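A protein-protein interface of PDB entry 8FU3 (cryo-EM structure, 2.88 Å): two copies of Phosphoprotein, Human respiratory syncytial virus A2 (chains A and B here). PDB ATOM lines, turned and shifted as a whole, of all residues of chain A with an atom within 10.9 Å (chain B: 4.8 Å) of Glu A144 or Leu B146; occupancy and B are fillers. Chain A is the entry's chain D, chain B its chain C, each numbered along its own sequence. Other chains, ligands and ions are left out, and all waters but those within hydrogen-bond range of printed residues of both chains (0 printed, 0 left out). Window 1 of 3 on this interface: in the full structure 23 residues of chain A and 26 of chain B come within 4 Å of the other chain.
The side-chain sulfur (SD) of Met A148 lies close to the backbone NH (N) of His B150, 3.5 Å away.
CG2 of Ile A138 touches CD1 of Leu B142 (3.6 Å).
Lys A141 touches Leu B142 (CD to CB, 3.8 Å).
CE of Lys A141 touches OG of Ser B143, at 3.4 Å.
Leu B146 touches Lys A141 (CD1 to CG, 3.7 Å).
Leu A142 touches Leu B142.
CB of Glu A144 touches CD2 of Leu B146, at 3.7 Å.
Ile A145 touches Ile B145 (CD1 to CG2, 3.9 Å).
CG1 of Ile A145 touches CD2 of Leu B146 (3.4 Å).
Leu B149 touches Met A148.
CD2 of Leu B149 touches CD2 of Leu A149 (3.8 Å).
Of chain B, only Leu B146 (3.7 Å) comes within 4 Å of Glu A144.
Leu B146 touches four residues of chain A.
Printed residues of chain A within 4 Å of Ser B143: Lys A141 (3.4 Å).
Ile B145 touches just one residue of chain A: Ile A145 (3.9 Å).
Of chain A, only Met A148 (3.5 Å) comes within 4 Å of His B150.
Of the printed residues of chain B, Ile A138 touches Leu B142.
Printed residues of chain B within 4 Å of Met A148: Leu B146, Leu B149 and His B150.
Printed residues of chain B within 4 Å of Lys A141: Leu B142 (3.8 Å), Ser B143 (3.4 Å) and Leu B146 (3.7 Å).
Of the printed residues of chain B, Ile A145 touches Leu B142 (3.6 Å), Ile B145 (3.9 Å), Leu B146 (3.4 Å) and Leu B149 (3.6 Å).
The nearest printed residue of chain B that does not touch Ile A138 is Leu B146 (7.4 Å).
Of the 18 printed residues of chain A, 7 touch a printed residue of chain B.
Along chain A the printed residues that touch a printed residue of chain B span positions 138 to 149.
Hydrophobic or aromatic side chains of chain B that line the printed part of chain A: Leu B142, Ile B145, Leu B146, Leu B149 and His B150.
Along chain B the printed residues that touch a printed residue of chain A span positions 142 to 150.
Among the printed residues, 14 pairs touch across the chains.
Among the printed residues, no Asp or Glu carboxylate lies within 4 Å of a Lys or Arg side-chain nitrogen of the other chain.
Ile A145 touches Leu B146, but with the chains exchanged Leu A146 does not touch Ile B145 (7.8 Å).
Ile A145 touches Leu B149, but with the chains exchanged Leu A149 does not touch Ile B145 (6.7 Å).
Met A148 touches Leu B146, but with the chains exchanged Leu A146 does not touch Met B148 (11.2 Å).
Met A148 touches His B150, but with the chains exchanged His A150 does not touch Met B148 (12.2 Å).
Positions printed for both chains: 142, 143, 144, 145, 146, 147, 148, 149, 150 and 151.
Of the 14 pairs that touch across the chains among the printed residues, 3 have their exchanged pair printed and touching as well.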
ATOM      1  N   ASP A 136     -35.337 -24.097   9.283  1.00  0.00           N
ATOM      2  CA  ASP A 136     -35.997 -23.327   8.236  1.00  0.00           C
ATOM      3  C   ASP A 136     -34.996 -22.439   7.510  1.00  0.00           C
ATOM      4  O   ASP A 136     -35.031 -22.323   6.282  1.00  0.00           O
ATOM      5  CB  ASP A 136     -37.110 -22.449   8.818  1.00  0.00           C
ATOM      6  CG  ASP A 136     -38.358 -23.215   9.258  1.00  0.00           C
ATOM      7  OD1 ASP A 136     -38.499 -24.364   8.912  1.00  0.00           O
ATOM      8  OD2 ASP A 136     -39.169 -22.625   9.931  1.00  0.00           O
ATOM      9  N   ARG A 137     -34.080 -21.839   8.265  1.00  0.00           N
ATOM     10  CA  ARG A 137     -33.056 -20.994   7.670  1.00  0.00           C
ATOM     11  C   ARG A 137     -32.091 -21.822   6.832  1.00  0.00           C
ATOM     12  O   ARG A 137     -31.616 -21.376   5.787  1.00  0.00           O
ATOM     13  CB  ARG A 137     -32.297 -20.225   8.738  1.00  0.00           C
ATOM     14  CG  ARG A 137     -33.120 -19.166   9.490  1.00  0.00           C
ATOM     15  CD  ARG A 137     -33.602 -18.074   8.591  1.00  0.00           C
ATOM     16  NE  ARG A 137     -34.228 -16.991   9.335  1.00  0.00           N
ATOM     17  CZ  ARG A 137     -34.910 -15.969   8.774  1.00  0.00           C
ATOM     18  NH1 ARG A 137     -35.048 -15.904   7.466  1.00  0.00           N
ATOM     19  NH2 ARG A 137     -35.449 -15.033   9.540  1.00  0.00           N
ATOM     20  N   ILE A 138     -31.814 -23.038   7.263  1.00  0.00           N
ATOM     21  CA  ILE A 138     -30.958 -23.897   6.469  1.00  0.00           C
ATOM     22  C   ILE A 138     -31.604 -24.209   5.135  1.00  0.00           C
ATOM     23  O   ILE A 138     -30.947 -24.146   4.096  1.00  0.00           O
ATOM     24  CB  ILE A 138     -30.607 -25.188   7.214  1.00  0.00           C
ATOM     25  CG1 ILE A 138     -29.659 -24.858   8.373  1.00  0.00           C
ATOM     26  CG2 ILE A 138     -29.999 -26.184   6.255  1.00  0.00           C
ATOM     27  CD1 ILE A 138     -29.472 -25.988   9.371  1.00  0.00           C
ATOM     28  N   ASP A 139     -32.891 -24.528   5.147  1.00  0.00           N
ATOM     29  CA  ASP A 139     -33.567 -24.852   3.901  1.00  0.00           C
ATOM     30  C   ASP A 139     -33.479 -23.719   2.887  1.00  0.00           C
ATOM     31  O   ASP A 139     -33.229 -23.965   1.705  1.00  0.00           O
ATOM     32  CB  ASP A 139     -35.037 -25.192   4.150  1.00  0.00           C
ATOM     33  CG  ASP A 139     -35.254 -26.575   4.778  1.00  0.00           C
ATOM     34  OD1 ASP A 139     -34.359 -27.383   4.745  1.00  0.00           O
ATOM     35  OD2 ASP A 139     -36.331 -26.807   5.279  1.00  0.00           O
ATOM     36  N   GLU A 140     -33.659 -22.473   3.328  1.00  0.00           N
ATOM     37  CA  GLU A 140     -33.577 -21.371   2.375  1.00  0.00           C
ATOM     38  C   GLU A 140     -32.144 -21.147   1.900  1.00  0.00           C
ATOM     39  O   GLU A 140     -31.929 -20.751   0.755  1.00  0.00           O
ATOM     40  CB  GLU A 140     -34.177 -20.079   2.947  1.00  0.00           C
ATOM     41  CG  GLU A 140     -33.423 -19.473   4.085  1.00  0.00           C
ATOM     42  CD  GLU A 140     -34.142 -18.316   4.720  1.00  0.00           C
ATOM     43  OE1 GLU A 140     -35.197 -17.962   4.255  1.00  0.00           O
ATOM     44  OE2 GLU A 140     -33.629 -17.782   5.674  1.00  0.00           O
ATOM     45  N   LYS A 141     -31.161 -21.437   2.750  1.00  0.00           N
ATOM     46  CA  LYS A 141     -29.775 -21.317   2.317  1.00  0.00           C
ATOM     47  C   LYS A 141     -29.469 -22.350   1.250  1.00  0.00           C
ATOM     48  O   LYS A 141     -28.810 -22.052   0.256  1.00  0.00           O
ATOM     49  CB  LYS A 141     -28.803 -21.479   3.482  1.00  0.00           C
ATOM     50  CG  LYS A 141     -28.736 -20.291   4.410  1.00  0.00           C
ATOM     51  CD  LYS A 141     -27.599 -20.446   5.407  1.00  0.00           C
ATOM     52  CE  LYS A 141     -27.414 -19.187   6.233  1.00  0.00           C
ATOM     53  NZ  LYS A 141     -28.534 -18.977   7.168  1.00  0.00           N
ATOM     54  N   LEU A 142     -29.978 -23.560   1.440  1.00  0.00           N
ATOM     55  CA  LEU A 142     -29.761 -24.628   0.480  1.00  0.00           C
ATOM     56  C   LEU A 142     -30.414 -24.275  -0.842  1.00  0.00           C
ATOM     57  O   LEU A 142     -29.870 -24.560  -1.909  1.00  0.00           O
ATOM     58  CB  LEU A 142     -30.332 -25.931   1.020  1.00  0.00           C
ATOM     59  CG  LEU A 142     -29.625 -26.506   2.248  1.00  0.00           C
ATOM     60  CD1 LEU A 142     -30.481 -27.575   2.840  1.00  0.00           C
ATOM     61  CD2 LEU A 142     -28.277 -27.086   1.856  1.00  0.00           C
ATOM     62  N   SER A 143     -31.575 -23.633  -0.768  1.00  0.00           N
ATOM     63  CA  SER A 143     -32.273 -23.197  -1.966  1.00  0.00           C
ATOM     64  C   SER A 143     -31.424 -22.197  -2.735  1.00  0.00           C
ATOM     65  O   SER A 143     -31.274 -22.306  -3.955  1.00  0.00           O
ATOM     66  CB  SER A 143     -33.604 -22.574  -1.602  1.00  0.00           C
ATOM     67  OG  SER A 143     -34.293 -22.154  -2.747  1.00  0.00           O
ATOM     68  N   GLU A 144     -30.834 -21.243  -2.016  1.00  0.00           N
ATOM     69  CA  GLU A 144     -29.966 -20.253  -2.641  1.00  0.00           C
ATOM     70  C   GLU A 144     -28.729 -20.903  -3.241  1.00  0.00           C
ATOM     71  O   GLU A 144     -28.291 -20.522  -4.326  1.00  0.00           O
ATOM     72  CB  GLU A 144     -29.534 -19.198  -1.625  1.00  0.00           C
ATOM     73  CG  GLU A 144     -30.620 -18.239  -1.196  1.00  0.00           C
ATOM     74  CD  GLU A 144     -31.049 -17.311  -2.290  1.00  0.00           C
ATOM     75  OE1 GLU A 144     -30.197 -16.700  -2.889  1.00  0.00           O
ATOM     76  OE2 GLU A 144     -32.228 -17.211  -2.534  1.00  0.00           O
ATOM     77  N   ILE A 145     -28.184 -21.902  -2.553  1.00  0.00           N
ATOM     78  CA  ILE A 145     -27.014 -22.597  -3.063  1.00  0.00           C
ATOM     79  C   ILE A 145     -27.334 -23.293  -4.366  1.00  0.00           C
ATOM     80  O   ILE A 145     -26.585 -23.180  -5.337  1.00  0.00           O
ATOM     81  CB  ILE A 145     -26.470 -23.622  -2.051  1.00  0.00           C
ATOM     82  CG1 ILE A 145     -25.861 -22.895  -0.859  1.00  0.00           C
ATOM     83  CG2 ILE A 145     -25.467 -24.530  -2.714  1.00  0.00           C
ATOM     84  CD1 ILE A 145     -25.547 -23.779   0.328  1.00  0.00           C
ATOM     85  N   LEU A 146     -28.453 -23.998  -4.401  1.00  0.00           N
ATOM     86  CA  LEU A 146     -28.854 -24.674  -5.617  1.00  0.00           C
ATOM     87  C   LEU A 146     -29.171 -23.674  -6.708  1.00  0.00           C
ATOM     88  O   LEU A 146     -28.827 -23.894  -7.867  1.00  0.00           O
ATOM     89  CB  LEU A 146     -30.054 -25.580  -5.350  1.00  0.00           C
ATOM     90  CG  LEU A 146     -29.749 -26.846  -4.533  1.00  0.00           C
ATOM     91  CD1 LEU A 146     -31.046 -27.490  -4.089  1.00  0.00           C
ATOM     92  CD2 LEU A 146     -28.945 -27.827  -5.404  1.00  0.00           C
ATOM     93  N   GLY A 147     -29.791 -22.559  -6.344  1.00  0.00           N
ATOM     94  CA  GLY A 147     -30.104 -21.527  -7.321  1.00  0.00           C
ATOM     95  C   GLY A 147     -28.834 -21.054  -8.016  1.00  0.00           C
ATOM     96  O   GLY A 147     -28.772 -20.987  -9.247  1.00  0.00           O
ATOM     97  N   MET A 148     -27.816 -20.730  -7.221  1.00  0.00           N
ATOM     98  CA  MET A 148     -26.547 -20.275  -7.766  1.00  0.00           C
ATOM     99  C   MET A 148     -25.866 -21.360  -8.583  1.00  0.00           C
ATOM    100  O   MET A 148     -25.303 -21.080  -9.640  1.00  0.00           O
ATOM    101  CB  MET A 148     -25.637 -19.804  -6.646  1.00  0.00           C
ATOM    102  CG  MET A 148     -26.076 -18.507  -6.015  1.00  0.00           C
ATOM    103  SD  MET A 148     -24.864 -17.849  -4.894  1.00  0.00           S
ATOM    104  CE  MET A 148     -24.996 -18.954  -3.514  1.00  0.00           C
ATOM    105  N   LEU A 149     -25.929 -22.599  -8.114  1.00  0.00           N
ATOM    106  CA  LEU A 149     -25.324 -23.683  -8.866  1.00  0.00           C
ATOM    107  C   LEU A 149     -26.068 -23.940 -10.157  1.00  0.00           C
ATOM    108  O   LEU A 149     -25.449 -24.231 -11.175  1.00  0.00           O
ATOM    109  CB  LEU A 149     -25.246 -24.950  -8.028  1.00  0.00           C
ATOM    110  CG  LEU A 149     -24.212 -24.925  -6.907  1.00  0.00           C
ATOM    111  CD1 LEU A 149     -24.420 -26.095  -6.014  1.00  0.00           C
ATOM    112  CD2 LEU A 149     -22.803 -24.989  -7.499  1.00  0.00           C
ATOM    113  N   HIS A 150     -27.384 -23.792 -10.148  1.00  0.00           N
ATOM    114  CA  HIS A 150     -28.121 -23.947 -11.388  1.00  0.00           C
ATOM    115  C   HIS A 150     -27.671 -22.874 -12.354  1.00  0.00           C
ATOM    116  O   HIS A 150     -27.440 -23.141 -13.529  1.00  0.00           O
ATOM    117  CB  HIS A 150     -29.631 -23.840 -11.167  1.00  0.00           C
ATOM    118  CG  HIS A 150     -30.268 -25.080 -10.624  1.00  0.00           C
ATOM    119  ND1 HIS A 150     -30.341 -26.251 -11.349  1.00  0.00           N
ATOM    120  CD2 HIS A 150     -30.873 -25.335  -9.442  1.00  0.00           C
ATOM    121  CE1 HIS A 150     -30.964 -27.167 -10.634  1.00  0.00           C
ATOM    122  NE2 HIS A 150     -31.296 -26.639  -9.474  1.00  0.00           N
ATOM    123  N   THR A 151     -27.494 -21.664 -11.845  1.00  0.00           N
ATOM    124  CA  THR A 151     -27.033 -20.575 -12.685  1.00  0.00           C
ATOM    125  C   THR A 151     -25.663 -20.887 -13.267  1.00  0.00           C
ATOM    126  O   THR A 151     -25.437 -20.717 -14.463  1.00  0.00           O
ATOM    127  CB  THR A 151     -26.960 -19.260 -11.886  1.00  0.00           C
ATOM    128  OG1 THR A 151     -28.268 -18.910 -11.423  1.00  0.00           O
ATOM    129  CG2 THR A 151     -26.406 -18.137 -12.749  1.00  0.00           C
ATOM    130  N   LEU A 152     -24.750 -21.348 -12.417  1.00  0.00           N
ATOM    131  CA  LEU A 152     -23.388 -21.637 -12.844  1.00  0.00           C
ATOM    132  C   LEU A 152     -23.303 -22.813 -13.799  1.00  0.00           C
ATOM    133  O   LEU A 152     -22.575 -22.752 -14.789  1.00  0.00           O
ATOM    134  CB  LEU A 152     -22.516 -21.931 -11.622  1.00  0.00           C
ATOM    135  CG  LEU A 152     -22.186 -20.751 -10.725  1.00  0.00           C
ATOM    136  CD1 LEU A 152     -21.659 -21.252  -9.397  1.00  0.00           C
ATOM    137  CD2 LEU A 152     -21.132 -19.891 -11.402  1.00  0.00           C
ATOM    138  N   VAL A 153     -24.036 -23.882 -13.507  1.00  0.00           N
ATOM    139  CA  VAL A 153     -24.004 -25.074 -14.343  1.00  0.00           C
ATOM    140  C   VAL A 153     -24.642 -24.789 -15.683  1.00  0.00           C
ATOM    141  O   VAL A 153     -24.152 -25.233 -16.721  1.00  0.00           O
ATOM    142  CB  VAL A 153     -24.708 -26.257 -13.655  1.00  0.00           C
ATOM    143  CG1 VAL A 153     -24.837 -27.428 -14.624  1.00  0.00           C
ATOM    144  CG2 VAL A 153     -23.901 -26.688 -12.436  1.00  0.00           C
ATOM    145  N   LEU B 142     -22.681 -23.291   5.656  1.00  0.00           N
ATOM    146  CA  LEU B 142     -23.528 -22.939   4.535  1.00  0.00           C
ATOM    147  C   LEU B 142     -23.317 -21.485   4.152  1.00  0.00           C
ATOM    148  O   LEU B 142     -23.270 -21.158   2.967  1.00  0.00           O
ATOM    149  CB  LEU B 142     -24.985 -23.200   4.887  1.00  0.00           C
ATOM    150  CG  LEU B 142     -25.371 -24.668   5.003  1.00  0.00           C
ATOM    151  CD1 LEU B 142     -26.691 -24.777   5.685  1.00  0.00           C
ATOM    152  CD2 LEU B 142     -25.464 -25.286   3.618  1.00  0.00           C
ATOM    153  N   SER B 143     -23.155 -20.613   5.147  1.00  0.00           N
ATOM    154  CA  SER B 143     -22.908 -19.202   4.876  1.00  0.00           C
ATOM    155  C   SER B 143     -21.595 -19.023   4.133  1.00  0.00           C
ATOM    156  O   SER B 143     -21.510 -18.241   3.183  1.00  0.00           O
ATOM    157  CB  SER B 143     -22.877 -18.413   6.164  1.00  0.00           C
ATOM    158  OG  SER B 143     -24.134 -18.381   6.768  1.00  0.00           O
ATOM    159  N   GLU B 144     -20.577 -19.764   4.550  1.00  0.00           N
ATOM    160  CA  GLU B 144     -19.284 -19.721   3.886  1.00  0.00           C
ATOM    161  C   GLU B 144     -19.412 -20.230   2.456  1.00  0.00           C
ATOM    162  O   GLU B 144     -18.836 -19.656   1.532  1.00  0.00           O
ATOM    163  CB  GLU B 144     -18.261 -20.542   4.666  1.00  0.00           C
ATOM    164  CG  GLU B 144     -16.849 -20.477   4.131  1.00  0.00           C
ATOM    165  CD  GLU B 144     -15.878 -21.197   5.000  1.00  0.00           C
ATOM    166  OE1 GLU B 144     -16.205 -21.459   6.130  1.00  0.00           O
ATOM    167  OE2 GLU B 144     -14.805 -21.499   4.541  1.00  0.00           O
ATOM    168  N   ILE B 145     -20.195 -21.288   2.272  1.00  0.00           N
ATOM    169  CA  ILE B 145     -20.438 -21.834   0.947  1.00  0.00           C
ATOM    170  C   ILE B 145     -21.153 -20.817   0.080  1.00  0.00           C
ATOM    171  O   ILE B 145     -20.797 -20.634  -1.085  1.00  0.00           O
ATOM    172  CB  ILE B 145     -21.268 -23.131   1.004  1.00  0.00           C
ATOM    173  CG1 ILE B 145     -20.437 -24.254   1.632  1.00  0.00           C
ATOM    174  CG2 ILE B 145     -21.739 -23.512  -0.392  1.00  0.00           C
ATOM    175  CD1 ILE B 145     -21.227 -25.494   1.999  1.00  0.00           C
ATOM    176  N   LEU B 146     -22.155 -20.155   0.643  1.00  0.00           N
ATOM    177  CA  LEU B 146     -22.892 -19.143  -0.092  1.00  0.00           C
ATOM    178  C   LEU B 146     -21.969 -18.017  -0.518  1.00  0.00           C
ATOM    179  O   LEU B 146     -22.052 -17.526  -1.645  1.00  0.00           O
ATOM    180  CB  LEU B 146     -24.027 -18.586   0.776  1.00  0.00           C
ATOM    181  CG  LEU B 146     -25.241 -19.506   0.999  1.00  0.00           C
ATOM    182  CD1 LEU B 146     -26.069 -18.985   2.135  1.00  0.00           C
ATOM    183  CD2 LEU B 146     -26.089 -19.525  -0.250  1.00  0.00           C
ATOM    184  N   GLY B 147     -21.070 -17.623   0.373  1.00  0.00           N
ATOM    185  CA  GLY B 147     -20.107 -16.580   0.071  1.00  0.00           C
ATOM    186  C   GLY B 147     -19.256 -16.957  -1.128  1.00  0.00           C
ATOM    187  O   GLY B 147     -19.107 -16.183  -2.078  1.00  0.00           O
ATOM    188  N   MET B 148     -18.698 -18.157  -1.077  1.00  0.00           N
ATOM    189  CA  MET B 148     -17.836 -18.631  -2.141  1.00  0.00           C
ATOM    190  C   MET B 148     -18.596 -18.707  -3.451  1.00  0.00           C
ATOM    191  O   MET B 148     -18.117 -18.235  -4.482  1.00  0.00           O
ATOM    192  CB  MET B 148     -17.304 -20.015  -1.778  1.00  0.00           C
ATOM    193  CG  MET B 148     -16.375 -20.038  -0.569  1.00  0.00           C
ATOM    194  SD  MET B 148     -14.784 -19.292  -0.860  1.00  0.00           S
ATOM    195  CE  MET B 148     -13.957 -20.648  -1.665  1.00  0.00           C
ATOM    196  N   LEU B 149     -19.783 -19.296  -3.420  1.00  0.00           N
ATOM    197  CA  LEU B 149     -20.539 -19.475  -4.642  1.00  0.00           C
ATOM    198  C   LEU B 149     -21.023 -18.168  -5.216  1.00  0.00           C
ATOM    199  O   LEU B 149     -21.035 -17.998  -6.432  1.00  0.00           O
ATOM    200  CB  LEU B 149     -21.728 -20.393  -4.407  1.00  0.00           C
ATOM    201  CG  LEU B 149     -21.406 -21.854  -4.153  1.00  0.00           C
ATOM    202  CD1 LEU B 149     -22.658 -22.545  -3.747  1.00  0.00           C
ATOM    203  CD2 LEU B 149     -20.839 -22.499  -5.414  1.00  0.00           C
ATOM    204  N   HIS B 150     -21.416 -17.237  -4.367  1.00  0.00           N
ATOM    205  CA  HIS B 150     -21.887 -15.974  -4.898  1.00  0.00           C
ATOM    206  C   HIS B 150     -20.758 -15.228  -5.574  1.00  0.00           C
ATOM    207  O   HIS B 150     -20.937 -14.666  -6.652  1.00  0.00           O
ATOM    208  CB  HIS B 150     -22.520 -15.104  -3.831  1.00  0.00           C
ATOM    209  CG  HIS B 150     -23.050 -13.858  -4.415  1.00  0.00           C
ATOM    210  ND1 HIS B 150     -23.964 -13.857  -5.441  1.00  0.00           N
ATOM    211  CD2 HIS B 150     -22.800 -12.572  -4.135  1.00  0.00           C
ATOM    212  CE1 HIS B 150     -24.240 -12.619  -5.776  1.00  0.00           C
ATOM    213  NE2 HIS B 150     -23.549 -11.817  -5.000  1.00  0.00           N
ATOM    214  N   THR B 151     -19.583 -15.226  -4.953  1.00  0.00           N
ATOM    215  CA  THR B 151     -18.449 -14.566  -5.573  1.00  0.00           C
ATOM    216  C   THR B 151     -18.173 -15.220  -6.911  1.00  0.00           C
ATOM    217  O   THR B 151     -17.892 -14.543  -7.900  1.00  0.00           O
ATOM    218  CB  THR B 151     -17.194 -14.635  -4.704  1.00  0.00           C
ATOM    219  OG1 THR B 151     -17.444 -13.985  -3.457  1.00  0.00           O
ATOM    220  CG2 THR B 151     -16.049 -13.934  -5.423  1.00  0.00           C
